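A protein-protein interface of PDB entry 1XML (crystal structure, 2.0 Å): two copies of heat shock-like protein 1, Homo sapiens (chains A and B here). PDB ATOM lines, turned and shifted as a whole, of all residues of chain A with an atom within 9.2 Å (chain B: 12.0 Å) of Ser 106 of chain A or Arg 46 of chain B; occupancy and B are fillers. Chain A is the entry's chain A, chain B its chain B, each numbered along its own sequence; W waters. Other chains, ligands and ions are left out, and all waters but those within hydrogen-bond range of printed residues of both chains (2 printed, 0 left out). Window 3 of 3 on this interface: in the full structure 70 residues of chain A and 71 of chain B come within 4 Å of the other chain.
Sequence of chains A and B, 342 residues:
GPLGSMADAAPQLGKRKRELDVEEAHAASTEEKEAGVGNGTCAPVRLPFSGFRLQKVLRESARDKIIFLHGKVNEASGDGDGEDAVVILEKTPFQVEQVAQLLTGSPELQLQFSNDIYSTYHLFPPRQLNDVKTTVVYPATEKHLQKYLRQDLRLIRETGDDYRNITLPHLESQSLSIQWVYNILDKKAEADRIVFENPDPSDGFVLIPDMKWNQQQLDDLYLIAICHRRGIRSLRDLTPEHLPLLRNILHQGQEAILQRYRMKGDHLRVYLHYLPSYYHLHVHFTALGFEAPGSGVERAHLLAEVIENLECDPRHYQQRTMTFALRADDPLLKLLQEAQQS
The backbone NH (N) of Phe 124 of chain A sits at hydrogen-bond distance from the backbone carbonyl oxygen (O) of Glu 108 of chain A (3.0 Å). The side-chain hydroxyl (OG) of Ser 119 of chain A lies close to the side-chain hydroxyl (OH) of Tyr 121 of chain A (3.4 Å).
The side-chain hydroxyl of Ser 106 of chain A is in hydrogen-bond range of the guanidinium group of Arg 46 of chain B (3.4 Å). The backbone NH (N) of Phe 52 of chain B is in hydrogen-bond range of the side-chain hydroxyl (OG1) of Thr 104 of chain A, 3.3 Å away. OE1 of Glu 108 of chain A lies within salt-bridge range of NE of Arg 127 of chain B (3.2 Å). N of Tyr 121 of chain A sits at hydrogen-bond distance from O of Thr 134 of chain B, at 2.9 Å. O of Ser 119 of chain A is in hydrogen-bond range of N of Val 136 of chain B (2.9 Å).
Water W2 lies within hydrogen-bond range of the side-chain hydroxyl (OG) of Ser 119 of chain A and the backbone carbonyl oxygen (O) of Val 136 of chain B. Water W1 bridges O of Phe 49 of chain B (3.1 Å) and O of Gly 105 of chain A (3.5 Å).
CD1 of Leu 103 of chain A touches CE2 of Phe 52 of chain B (3.8 Å). Leu 103 of chain A touches Val 87 of chain B (CD1 to CG1, 3.8 Å). Val 45 of chain B touches Pro 107 of chain A (O to O, 3.9 Å). O of Val 45 of chain B touches CD1 of Leu 109 of chain A, at 3.2 Å. CD1 of Leu 47 of chain B touches CD2 of Leu 109 of chain A, 3.6 Å away. Thr 134 of chain B touches Ser 119 of chain A (O to O, 3.8 Å). Tyr 121 of chain A touches Pro 48 of chain B. CD2 of Leu 123 of chain A touches CD1 of Leu 89 of chain B, 3.9 Å away. Leu 123 of chain A touches Thr 134 of chain B. Phe 124 of chain A touches Arg 127 of chain B.
No position is printed for both chains. Of the 19 pairs that touch across the chains among the printed residues, none has its exchanged pair printed and touching as well.
Printed residues of chain B that touch a printed residue of chain A: Val 45, Arg 46, Leu 47, Pro 48, Phe 52, Val 87, Leu 89, Arg 127, Thr 134, Thr 135 and Val 136. Of the 18 printed residues of chain A, 10 touch a printed residue of chain B. Hydrophobic or aromatic side chains of chain A within 4 Å of the printed part of chain B: Leu 103, Pro 107, Leu 109, Tyr 121, Leu 123 and Phe 124. Among the printed residues, 19 pairs touch across the chains.
Thr 104 of chain A touches just one residue of chain B: Phe 52. No residue of chain B comes within 4 Å of Gly 105 of chain A. Of chain B, only Val 45 (3.9 Å) and Leu 47 (3.7 Å) come within 4 Å of Pro 107 of chain A. Pro 125 of chain A touches none of the printed residues of chain B. Of chain A, only Pro 107 and Leu 109 come within 4 Å of Val 45 of chain B. Of chain A, only Ser 106 and Leu 109 come within 4 Å of Arg 46 of chain B. Ser 50 of chain B touches none of the printed residues of chain A. Printed residues of chain A within 4 Å of Leu 89 of chain B: Leu 123. Of the printed residues of chain A, Thr 135 of chain B touches Ser 119. The nearest residue of chain A that does not touch Arg 46 of chain B is Tyr 121 of chain A (4.2 Å).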
ATOM      1  N   ALA A 100      14.315  -2.178 -13.143  1.00  0.00           N
ATOM      2  CA  ALA A 100      13.919  -3.507 -12.667  1.00  0.00           C
ATOM      3  C   ALA A 100      14.703  -4.612 -13.381  1.00  0.00           C
ATOM      4  O   ALA A 100      15.066  -5.618 -12.767  1.00  0.00           O
ATOM      5  CB  ALA A 100      12.417  -3.712 -12.850  1.00  0.00           C
ATOM      6  N   GLN A 101      14.965  -4.403 -14.670  1.00  0.00           N
ATOM      7  CA  GLN A 101      15.742  -5.333 -15.488  1.00  0.00           C
ATOM      8  C   GLN A 101      17.182  -5.479 -14.984  1.00  0.00           C
ATOM      9  O   GLN A 101      17.717  -6.587 -14.930  1.00  0.00           O
ATOM     10  CB  GLN A 101      15.745  -4.851 -16.946  1.00  0.00           C
ATOM     11  CG  GLN A 101      16.367  -5.821 -17.945  1.00  0.00           C
ATOM     12  CD  GLN A 101      15.437  -6.163 -19.099  1.00  0.00           C
ATOM     13  OE1 GLN A 101      15.244  -5.355 -20.008  1.00  0.00           O
ATOM     14  NE2 GLN A 101      14.861  -7.361 -19.063  1.00  0.00           N
ATOM     15  N   LEU A 102      17.794  -4.358 -14.605  1.00  0.00           N
ATOM     16  CA  LEU A 102      19.194  -4.329 -14.176  1.00  0.00           C
ATOM     17  C   LEU A 102      19.415  -4.993 -12.812  1.00  0.00           C
ATOM     18  O   LEU A 102      20.412  -5.685 -12.611  1.00  0.00           O
ATOM     19  CB  LEU A 102      19.700  -2.882 -14.134  1.00  0.00           C
ATOM     20  CG  LEU A 102      21.113  -2.655 -13.586  1.00  0.00           C
ATOM     21  CD1 LEU A 102      22.143  -3.267 -14.527  1.00  0.00           C
ATOM     22  CD2 LEU A 102      21.373  -1.171 -13.362  1.00  0.00           C
ATOM     23  N   LEU A 103      18.489  -4.768 -11.883  1.00  0.00           N
ATOM     24  CA  LEU A 103      18.618  -5.277 -10.515  1.00  0.00           C
ATOM     25  C   LEU A 103      18.345  -6.775 -10.416  1.00  0.00           C
ATOM     26  O   LEU A 103      18.841  -7.438  -9.500  1.00  0.00           O
ATOM     27  CB  LEU A 103      17.673  -4.524  -9.573  1.00  0.00           C
ATOM     28  CG  LEU A 103      17.940  -3.027  -9.413  1.00  0.00           C
ATOM     29  CD1 LEU A 103      16.917  -2.424  -8.476  1.00  0.00           C
ATOM     30  CD2 LEU A 103      19.349  -2.760  -8.906  1.00  0.00           C
ATOM     31  N   THR A 104      17.553  -7.300 -11.350  1.00  0.00           N
ATOM     32  CA  THR A 104      17.243  -8.727 -11.393  1.00  0.00           C
ATOM     33  C   THR A 104      18.442  -9.542 -11.892  1.00  0.00           C
ATOM     34  O   THR A 104      18.531 -10.742 -11.639  1.00  0.00           O
ATOM     35  CB  THR A 104      15.967  -8.986 -12.253  1.00  0.00           C
ATOM     36  OG1 THR A 104      15.233 -10.094 -11.716  1.00  0.00           O
ATOM     37  CG2 THR A 104      16.299  -9.410 -13.698  1.00  0.00           C
ATOM     38  N   GLY A 105      19.353  -8.886 -12.609  1.00  0.00           N
ATOM     39  CA  GLY A 105      20.604  -9.502 -13.021  1.00  0.00           C
ATOM     40  C   GLY A 105      21.680  -9.336 -11.960  1.00  0.00           C
ATOM     41  O   GLY A 105      21.418  -9.492 -10.762  1.00  0.00           O
ATOM     42  N   SER A 106      22.893  -9.011 -12.402  1.00  0.00           N
ATOM     43  CA  SER A 106      24.025  -8.805 -11.504  1.00  0.00           C
ATOM     44  C   SER A 106      24.682  -7.449 -11.789  1.00  0.00           C
ATOM     45  O   SER A 106      25.627  -7.360 -12.573  1.00  0.00           O
ATOM     46  CB  SER A 106      25.030  -9.948 -11.658  1.00  0.00           C
ATOM     47  OG  SER A 106      24.431 -11.190 -11.322  1.00  0.00           O
ATOM     48  N   PRO A 107      24.183  -6.392 -11.148  1.00  0.00           N
ATOM     49  CA  PRO A 107      24.710  -5.041 -11.378  1.00  0.00           C
ATOM     50  C   PRO A 107      26.118  -4.844 -10.815  1.00  0.00           C
ATOM     51  O   PRO A 107      26.536  -5.567  -9.908  1.00  0.00           O
ATOM     52  CB  PRO A 107      23.713  -4.121 -10.652  1.00  0.00           C
ATOM     53  CG  PRO A 107      22.658  -4.996 -10.063  1.00  0.00           C
ATOM     54  CD  PRO A 107      23.103  -6.408 -10.146  1.00  0.00           C
ATOM     55  N   GLU A 108      26.827  -3.862 -11.364  1.00  0.00           N
ATOM     56  CA  GLU A 108      28.169  -3.503 -10.920  1.00  0.00           C
ATOM     57  C   GLU A 108      28.022  -2.569  -9.728  1.00  0.00           C
ATOM     58  O   GLU A 108      27.553  -1.441  -9.886  1.00  0.00           O
ATOM     59  CB  GLU A 108      28.910  -2.793 -12.061  1.00  0.00           C
ATOM     60  CG  GLU A 108      30.422  -2.731 -11.916  1.00  0.00           C
ATOM     61  CD  GLU A 108      31.075  -1.869 -12.986  1.00  0.00           C
ATOM     62  OE1 GLU A 108      31.976  -1.076 -12.639  1.00  0.00           O
ATOM     63  OE2 GLU A 108      30.691  -1.976 -14.175  1.00  0.00           O
ATOM     64  N   LEU A 109      28.400  -3.028  -8.536  1.00  0.00           N
ATOM     65  CA  LEU A 109      28.244  -2.192  -7.344  1.00  0.00           C
ATOM     66  C   LEU A 109      29.423  -2.221  -6.373  1.00  0.00           C
ATOM     67  O   LEU A 109      30.185  -3.181  -6.323  1.00  0.00           O
ATOM     68  CB  LEU A 109      26.937  -2.522  -6.607  1.00  0.00           C
ATOM     69  CG  LEU A 109      26.573  -3.982  -6.339  1.00  0.00           C
ATOM     70  CD1 LEU A 109      27.093  -4.431  -4.978  1.00  0.00           C
ATOM     71  CD2 LEU A 109      25.061  -4.181  -6.428  1.00  0.00           C
ATOM     72  N   GLN A 110      29.550  -1.134  -5.616  1.00  0.00           N
ATOM     73  CA  GLN A 110      30.576  -0.959  -4.597  1.00  0.00           C
ATOM     74  C   GLN A 110      29.880  -0.485  -3.320  1.00  0.00           C
ATOM     75  O   GLN A 110      29.231   0.563  -3.317  1.00  0.00           O
ATOM     76  CB  GLN A 110      31.603   0.085  -5.049  1.00  0.00           C
ATOM     77  CG  GLN A 110      32.901   0.095  -4.230  1.00  0.00           C
ATOM     78  CD  GLN A 110      33.199   1.441  -3.574  1.00  0.00           C
ATOM     79  OE1 GLN A 110      33.718   2.354  -4.225  1.00  0.00           O
ATOM     80  NE2 GLN A 110      32.888   1.558  -2.283  1.00  0.00           N
ATOM     81  N   LEU A 111      29.993  -1.260  -2.249  1.00  0.00           N
ATOM     82  CA  LEU A 111      29.376  -0.886  -0.980  1.00  0.00           C
ATOM     83  C   LEU A 111      30.111   0.280  -0.317  1.00  0.00           C
ATOM     84  O   LEU A 111      31.287   0.170   0.030  1.00  0.00           O
ATOM     85  CB  LEU A 111      29.327  -2.079  -0.018  1.00  0.00           C
ATOM     86  CG  LEU A 111      28.572  -1.836   1.298  1.00  0.00           C
ATOM     87  CD1 LEU A 111      27.068  -1.840   1.073  1.00  0.00           C
ATOM     88  CD2 LEU A 111      28.967  -2.869   2.341  1.00  0.00           C
ATOM     89  N   SER A 119      21.662  -0.622   3.405  1.00  0.00           N
ATOM     90  CA  SER A 119      22.979  -0.673   2.787  1.00  0.00           C
ATOM     91  C   SER A 119      23.017   0.309   1.619  1.00  0.00           C
ATOM     92  O   SER A 119      22.033   0.452   0.891  1.00  0.00           O
ATOM     93  CB  SER A 119      23.281  -2.088   2.296  1.00  0.00           C
ATOM     94  OG  SER A 119      22.289  -2.510   1.379  1.00  0.00           O
ATOM     95  N   TYR A 121      25.260   1.903  -1.769  1.00  0.00           N
ATOM     96  CA  TYR A 121      26.207   1.505  -2.812  1.00  0.00           C
ATOM     97  C   TYR A 121      26.376   2.597  -3.882  1.00  0.00           C
ATOM     98  O   TYR A 121      25.505   3.458  -4.061  1.00  0.00           O
ATOM     99  CB  TYR A 121      25.708   0.257  -3.565  1.00  0.00           C
ATOM    100  CG  TYR A 121      25.323  -0.963  -2.750  1.00  0.00           C
ATOM    101  CD1 TYR A 121      24.015  -1.145  -2.299  1.00  0.00           C
ATOM    102  CD2 TYR A 121      26.252  -1.967  -2.485  1.00  0.00           C
ATOM    103  CE1 TYR A 121      23.651  -2.283  -1.575  1.00  0.00           C
ATOM    104  CE2 TYR A 121      25.901  -3.107  -1.758  1.00  0.00           C
ATOM    105  CZ  TYR A 121      24.603  -3.258  -1.311  1.00  0.00           C
ATOM    106  OH  TYR A 121      24.262  -4.377  -0.596  1.00  0.00           O
ATOM    107  N   LEU A 123      26.354   2.413  -7.839  1.00  0.00           N
ATOM    108  CA  LEU A 123      25.985   1.523  -8.921  1.00  0.00           C
ATOM    109  C   LEU A 123      26.518   2.139 -10.207  1.00  0.00           C
ATOM    110  O   LEU A 123      26.356   3.330 -10.440  1.00  0.00           O
ATOM    111  CB  LEU A 123      24.464   1.367  -8.978  1.00  0.00           C
ATOM    112  CG  LEU A 123      23.827   0.647 -10.167  1.00  0.00           C
ATOM    113  CD1 LEU A 123      24.511  -0.685 -10.449  1.00  0.00           C
ATOM    114  CD2 LEU A 123      22.339   0.442  -9.920  1.00  0.00           C
ATOM    115  N   PHE A 124      27.184   1.327 -11.019  1.00  0.00           N
ATOM    116  CA  PHE A 124      27.651   1.749 -12.334  1.00  0.00           C
ATOM    117  C   PHE A 124      26.843   0.948 -13.346  1.00  0.00           C
ATOM    118  O   PHE A 124      27.162  -0.207 -13.625  1.00  0.00           O
ATOM    119  CB  PHE A 124      29.153   1.508 -12.461  1.00  0.00           C
ATOM    120  CG  PHE A 124      29.969   2.347 -11.515  1.00  0.00           C
ATOM    121  CD1 PHE A 124      30.100   1.981 -10.179  1.00  0.00           C
ATOM    122  CD2 PHE A 124      30.585   3.514 -11.952  1.00  0.00           C
ATOM    123  CE1 PHE A 124      30.844   2.759  -9.292  1.00  0.00           C
ATOM    124  CE2 PHE A 124      31.331   4.298 -11.073  1.00  0.00           C
ATOM    125  CZ  PHE A 124      31.457   3.917  -9.736  1.00  0.00           C
ATOM    126  N   PRO A 125      25.763   1.543 -13.856  1.00  0.00           N
ATOM    127  CA  PRO A 125      24.839   0.814 -14.731  1.00  0.00           C
ATOM    128  C   PRO A 125      25.379   0.661 -16.148  1.00  0.00           C
ATOM    129  O   PRO A 125      26.359   1.323 -16.495  1.00  0.00           O
ATOM    130  CB  PRO A 125      23.569   1.681 -14.731  1.00  0.00           C
ATOM    131  CG  PRO A 125      23.877   2.911 -13.919  1.00  0.00           C
ATOM    132  CD  PRO A 125      25.343   2.943 -13.665  1.00  0.00           C
ATOM    133  N   PRO A 126      24.752  -0.191 -16.956  1.00  0.00           N
ATOM    134  CA  PRO A 126      25.115  -0.301 -18.374  1.00  0.00           C
ATOM    135  C   PRO A 126      24.779   0.983 -19.140  1.00  0.00           C
ATOM    136  O   PRO A 126      24.036   1.827 -18.625  1.00  0.00           O
ATOM    137  CB  PRO A 126      24.274  -1.486 -18.867  1.00  0.00           C
ATOM    138  CG  PRO A 126      23.144  -1.588 -17.911  1.00  0.00           C
ATOM    139  CD  PRO A 126      23.661  -1.111 -16.592  1.00  0.00           C
ATOM    140  N   VAL B  45      29.928  -6.523  -3.717  1.00  0.00           N
ATOM    141  CA  VAL B  45      29.926  -7.110  -5.091  1.00  0.00           C
ATOM    142  C   VAL B  45      28.494  -7.353  -5.563  1.00  0.00           C
ATOM    143  O   VAL B  45      28.121  -6.951  -6.664  1.00  0.00           O
ATOM    144  CB  VAL B  45      30.705  -8.449  -5.143  1.00  0.00           C
ATOM    145  CG1 VAL B  45      30.860  -8.941  -6.586  1.00  0.00           C
ATOM    146  CG2 VAL B  45      32.070  -8.312  -4.467  1.00  0.00           C
ATOM    147  N   ARG B  46      27.699  -8.005  -4.715  1.00  0.00           N
ATOM    148  CA  ARG B  46      26.328  -8.380  -5.058  1.00  0.00           C
ATOM    149  C   ARG B  46      25.330  -7.882  -4.020  1.00  0.00           C
ATOM    150  O   ARG B  46      25.696  -7.605  -2.877  1.00  0.00           O
ATOM    151  CB  ARG B  46      26.214  -9.900  -5.181  1.00  0.00           C
ATOM    152  CG  ARG B  46      27.365 -10.558  -5.938  1.00  0.00           C
ATOM    153  CD  ARG B  46      27.317 -12.073  -5.937  1.00  0.00           C
ATOM    154  NE  ARG B  46      25.969 -12.577  -6.189  1.00  0.00           N
ATOM    155  CZ  ARG B  46      25.363 -12.585  -7.376  1.00  0.00           C
ATOM    156  NH1 ARG B  46      25.972 -12.117  -8.461  1.00  0.00           N
ATOM    157  NH2 ARG B  46      24.130 -13.070  -7.479  1.00  0.00           N
ATOM    158  N   LEU B  47      24.068  -7.775  -4.431  1.00  0.00           N
ATOM    159  CA  LEU B  47      22.981  -7.392  -3.528  1.00  0.00           C
ATOM    160  C   LEU B  47      22.675  -8.538  -2.554  1.00  0.00           C
ATOM    161  O   LEU B  47      22.908  -9.701  -2.886  1.00  0.00           O
ATOM    162  CB  LEU B  47      21.726  -7.026  -4.327  1.00  0.00           C
ATOM    163  CG  LEU B  47      21.782  -5.681  -5.058  1.00  0.00           C
ATOM    164  CD1 LEU B  47      21.921  -5.887  -6.555  1.00  0.00           C
ATOM    165  CD2 LEU B  47      20.559  -4.823  -4.754  1.00  0.00           C
ATOM    166  N   PRO B  48      22.155  -8.216  -1.365  1.00  0.00           N
ATOM    167  CA  PRO B  48      21.875  -9.232  -0.332  1.00  0.00           C
ATOM    168  C   PRO B  48      20.793 -10.262  -0.699  1.00  0.00           C
ATOM    169  O   PRO B  48      20.670 -11.277  -0.008  1.00  0.00           O
ATOM    170  CB  PRO B  48      21.435  -8.397   0.884  1.00  0.00           C
ATOM    171  CG  PRO B  48      21.005  -7.089   0.340  1.00  0.00           C
ATOM    172  CD  PRO B  48      21.804  -6.858  -0.909  1.00  0.00           C
ATOM    173  N   PHE B  49      20.031  -9.999  -1.760  1.00  0.00           N
ATOM    174  CA  PHE B  49      19.035 -10.936  -2.276  1.00  0.00           C
ATOM    175  C   PHE B  49      19.327 -11.297  -3.734  1.00  0.00           C
ATOM    176  O   PHE B  49      20.098 -10.614  -4.408  1.00  0.00           O
ATOM    177  CB  PHE B  49      17.636 -10.323  -2.177  1.00  0.00           C
ATOM    178  CG  PHE B  49      17.530  -8.951  -2.788  1.00  0.00           C
ATOM    179  CD1 PHE B  49      17.432  -8.793  -4.167  1.00  0.00           C
ATOM    180  CD2 PHE B  49      17.542  -7.817  -1.986  1.00  0.00           C
ATOM    181  CE1 PHE B  49      17.342  -7.530  -4.730  1.00  0.00           C
ATOM    182  CE2 PHE B  49      17.450  -6.549  -2.547  1.00  0.00           C
ATOM    183  CZ  PHE B  49      17.349  -6.406  -3.917  1.00  0.00           C
ATOM    184  N   SER B  50      18.692 -12.369  -4.206  1.00  0.00           N
ATOM    185  CA  SER B  50      18.782 -12.801  -5.600  1.00  0.00           C
ATOM    186  C   SER B  50      17.407 -12.732  -6.263  1.00  0.00           C
ATOM    187  O   SER B  50      16.465 -13.386  -5.816  1.00  0.00           O
ATOM    188  CB  SER B  50      19.315 -14.232  -5.675  1.00  0.00           C
ATOM    189  OG  SER B  50      20.541 -14.353  -4.974  1.00  0.00           O
ATOM    190  N   GLY B  51      17.301 -11.941  -7.330  1.00  0.00           N
ATOM    191  CA  GLY B  51      16.042 -11.748  -8.034  1.00  0.00           C
ATOM    192  C   GLY B  51      15.338 -10.471  -7.610  1.00  0.00           C
ATOM    193  O   GLY B  51      15.510 -10.005  -6.480  1.00  0.00           O
ATOM    194  N   PHE B  52      14.540  -9.911  -8.514  1.00  0.00           N
ATOM    195  CA  PHE B  52      13.864  -8.638  -8.274  1.00  0.00           C
ATOM    196  C   PHE B  52      12.654  -8.442  -9.191  1.00  0.00           C
ATOM    197  O   PHE B  52      12.806  -8.305 -10.409  1.00  0.00           O
ATOM    198  CB  PHE B  52      14.844  -7.481  -8.469  1.00  0.00           C
ATOM    199  CG  PHE B  52      14.429  -6.220  -7.777  1.00  0.00           C
ATOM    200  CD1 PHE B  52      14.584  -6.093  -6.401  1.00  0.00           C
ATOM    201  CD2 PHE B  52      13.882  -5.166  -8.492  1.00  0.00           C
ATOM    202  CE1 PHE B  52      14.205  -4.934  -5.747  1.00  0.00           C
ATOM    203  CE2 PHE B  52      13.502  -4.002  -7.844  1.00  0.00           C
ATOM    204  CZ  PHE B  52      13.664  -3.887  -6.467  1.00  0.00           C
ATOM    205  N   VAL B  73      11.701 -10.088  -3.503  1.00  0.00           N
ATOM    206  CA  VAL B  73      12.990 -10.750  -3.701  1.00  0.00           C
ATOM    207  C   VAL B  73      12.993 -12.172  -3.143  1.00  0.00           C
ATOM    208  O   VAL B  73      12.217 -12.497  -2.244  1.00  0.00           O
ATOM    209  CB  VAL B  73      14.147  -9.917  -3.084  1.00  0.00           C
ATOM    210  CG1 VAL B  73      14.147  -8.507  -3.662  1.00  0.00           C
ATOM    211  CG2 VAL B  73      14.060  -9.870  -1.564  1.00  0.00           C
ATOM    212  N   ASN B  74      13.881 -13.002  -3.690  1.00  0.00           N
ATOM    213  CA  ASN B  74      13.948 -14.432  -3.380  1.00  0.00           C
ATOM    214  C   ASN B  74      12.649 -15.154  -3.720  1.00  0.00           C
ATOM    215  O   ASN B  74      12.649 -16.356  -3.974  1.00  0.00           O
ATOM    216  CB  ASN B  74      14.317 -14.679  -1.910  1.00  0.00           C
ATOM    217  CG  ASN B  74      15.613 -13.998  -1.505  1.00  0.00           C
ATOM    218  OD1 ASN B  74      16.266 -13.347  -2.319  1.00  0.00           O
ATOM    219  ND2 ASN B  74      15.993 -14.152  -0.241  1.00  0.00           N
ATOM    220  N   VAL B  87      14.325  -0.442  -2.959  1.00  0.00           N
ATOM    221  CA  VAL B  87      15.569   0.018  -3.558  1.00  0.00           C
ATOM    222  C   VAL B  87      15.379   1.427  -4.102  1.00  0.00           C
ATOM    223  O   VAL B  87      14.425   1.697  -4.837  1.00  0.00           O
ATOM    224  CB  VAL B  87      16.032  -0.914  -4.681  1.00  0.00           C
ATOM    225  CG1 VAL B  87      17.400  -0.478  -5.212  1.00  0.00           C
ATOM    226  CG2 VAL B  87      16.063  -2.359  -4.187  1.00  0.00           C
ATOM    227  N   LEU B  89      17.204   4.443  -6.192  1.00  0.00           N
ATOM    228  CA  LEU B  89      18.249   4.859  -7.130  1.00  0.00           C
ATOM    229  C   LEU B  89      18.187   6.379  -7.290  1.00  0.00           C
ATOM    230  O   LEU B  89      17.108   6.942  -7.474  1.00  0.00           O
ATOM    231  CB  LEU B  89      18.050   4.201  -8.498  1.00  0.00           C
ATOM    232  CG  LEU B  89      18.069   2.672  -8.677  1.00  0.00           C
ATOM    233  CD1 LEU B  89      19.288   2.037  -8.028  1.00  0.00           C
ATOM    234  CD2 LEU B  89      16.776   2.024  -8.165  1.00  0.00           C
ATOM    235  N   ARG B 127      32.458   5.637 -17.471  1.00  0.00           N
ATOM    236  CA  ARG B 127      31.986   5.071 -16.197  1.00  0.00           C
ATOM    237  C   ARG B 127      31.951   6.044 -14.997  1.00  0.00           C
ATOM    238  O   ARG B 127      31.112   5.905 -14.105  1.00  0.00           O
ATOM    239  CB  ARG B 127      32.852   3.834 -15.888  1.00  0.00           C
ATOM    240  CG  ARG B 127      32.850   3.283 -14.469  1.00  0.00           C
ATOM    241  CD  ARG B 127      34.033   2.340 -14.225  1.00  0.00           C
ATOM    242  NE  ARG B 127      33.868   1.479 -13.056  1.00  0.00           N
ATOM    243  CZ  ARG B 127      33.983   1.885 -11.790  1.00  0.00           C
ATOM    244  NH1 ARG B 127      34.265   3.155 -11.496  1.00  0.00           N
ATOM    245  NH2 ARG B 127      33.811   1.011 -10.802  1.00  0.00           N
ATOM    246  N   THR B 134      22.692   4.213  -4.581  1.00  0.00           N
ATOM    247  CA  THR B 134      21.732   3.121  -4.507  1.00  0.00           C
ATOM    248  C   THR B 134      21.569   2.649  -3.064  1.00  0.00           C
ATOM    249  O   THR B 134      22.461   2.015  -2.510  1.00  0.00           O
ATOM    250  CB  THR B 134      22.185   1.959  -5.422  1.00  0.00           C
ATOM    251  OG1 THR B 134      22.229   2.405  -6.789  1.00  0.00           O
ATOM    252  CG2 THR B 134      21.160   0.824  -5.430  1.00  0.00           C
ATOM    253  N   THR B 135      20.432   2.979  -2.457  1.00  0.00           N
ATOM    254  CA  THR B 135      20.112   2.551  -1.107  1.00  0.00           C
ATOM    255  C   THR B 135      19.167   1.347  -1.173  1.00  0.00           C
ATOM    256  O   THR B 135      18.219   1.339  -1.957  1.00  0.00           O
ATOM    257  CB  THR B 135      19.470   3.718  -0.320  1.00  0.00           C
ATOM    258  OG1 THR B 135      20.331   4.865  -0.372  1.00  0.00           O
ATOM    259  CG2 THR B 135      19.366   3.403   1.170  1.00  0.00           C
ATOM    260  N   VAL B 136      19.432   0.333  -0.356  1.00  0.00           N
ATOM    261  CA  VAL B 136      18.642  -0.897  -0.360  1.00  0.00           C
ATOM    262  C   VAL B 136      18.180  -1.219   1.054  1.00  0.00           C
ATOM    263  O   VAL B 136      18.939  -1.087   2.013  1.00  0.00           O
ATOM    264  CB  VAL B 136      19.443  -2.089  -0.938  1.00  0.00           C
ATOM    265  CG1 VAL B 136      18.595  -3.367  -0.951  1.00  0.00           C
ATOM    266  CG2 VAL B 136      19.941  -1.765  -2.335  1.00  0.00           C
ATOM    267  N   VAL B 137      16.925  -1.630   1.177  1.00  0.00           N
ATOM    268  CA  VAL B 137      16.338  -1.960   2.467  1.00  0.00           C
ATOM    269  C   VAL B 137      15.822  -3.383   2.376  1.00  0.00           C
ATOM    270  O   VAL B 137      14.919  -3.669   1.590  1.00  0.00           O
ATOM    271  CB  VAL B 137      15.202  -0.994   2.844  1.00  0.00           C
ATOM    272  CG1 VAL B 137      14.591  -1.372   4.213  1.00  0.00           C
ATOM    273  CG2 VAL B 137      15.715   0.446   2.860  1.00  0.00           C
ATOM    274  N   TYR B 138      16.414  -4.270   3.169  1.00  0.00           N
ATOM    275  CA  TYR B 138      16.093  -5.691   3.121  1.00  0.00           C
ATOM    276  C   TYR B 138      16.418  -6.365   4.462  1.00  0.00           C
ATOM    277  O   TYR B 138      17.555  -6.274   4.932  1.00  0.00           O
ATOM    278  CB  TYR B 138      16.864  -6.377   1.989  1.00  0.00           C
ATOM    279  CG  TYR B 138      16.683  -7.882   1.963  1.00  0.00           C
ATOM    280  CD1 TYR B 138      15.495  -8.455   1.507  1.00  0.00           C
ATOM    281  CD2 TYR B 138      17.690  -8.733   2.421  1.00  0.00           C
ATOM    282  CE1 TYR B 138      15.321  -9.837   1.495  1.00  0.00           C
ATOM    283  CE2 TYR B 138      17.523 -10.115   2.413  1.00  0.00           C
ATOM    284  CZ  TYR B 138      16.339 -10.661   1.947  1.00  0.00           C
ATOM    285  OH  TYR B 138      16.178 -12.028   1.935  1.00  0.00           O
HETATM  286  O   HOH W   1      20.688  -9.855  -7.404  1.00  0.00           O
HETATM  287  O   HOH W   2      20.095  -3.888   2.529  1.00  0.00           O
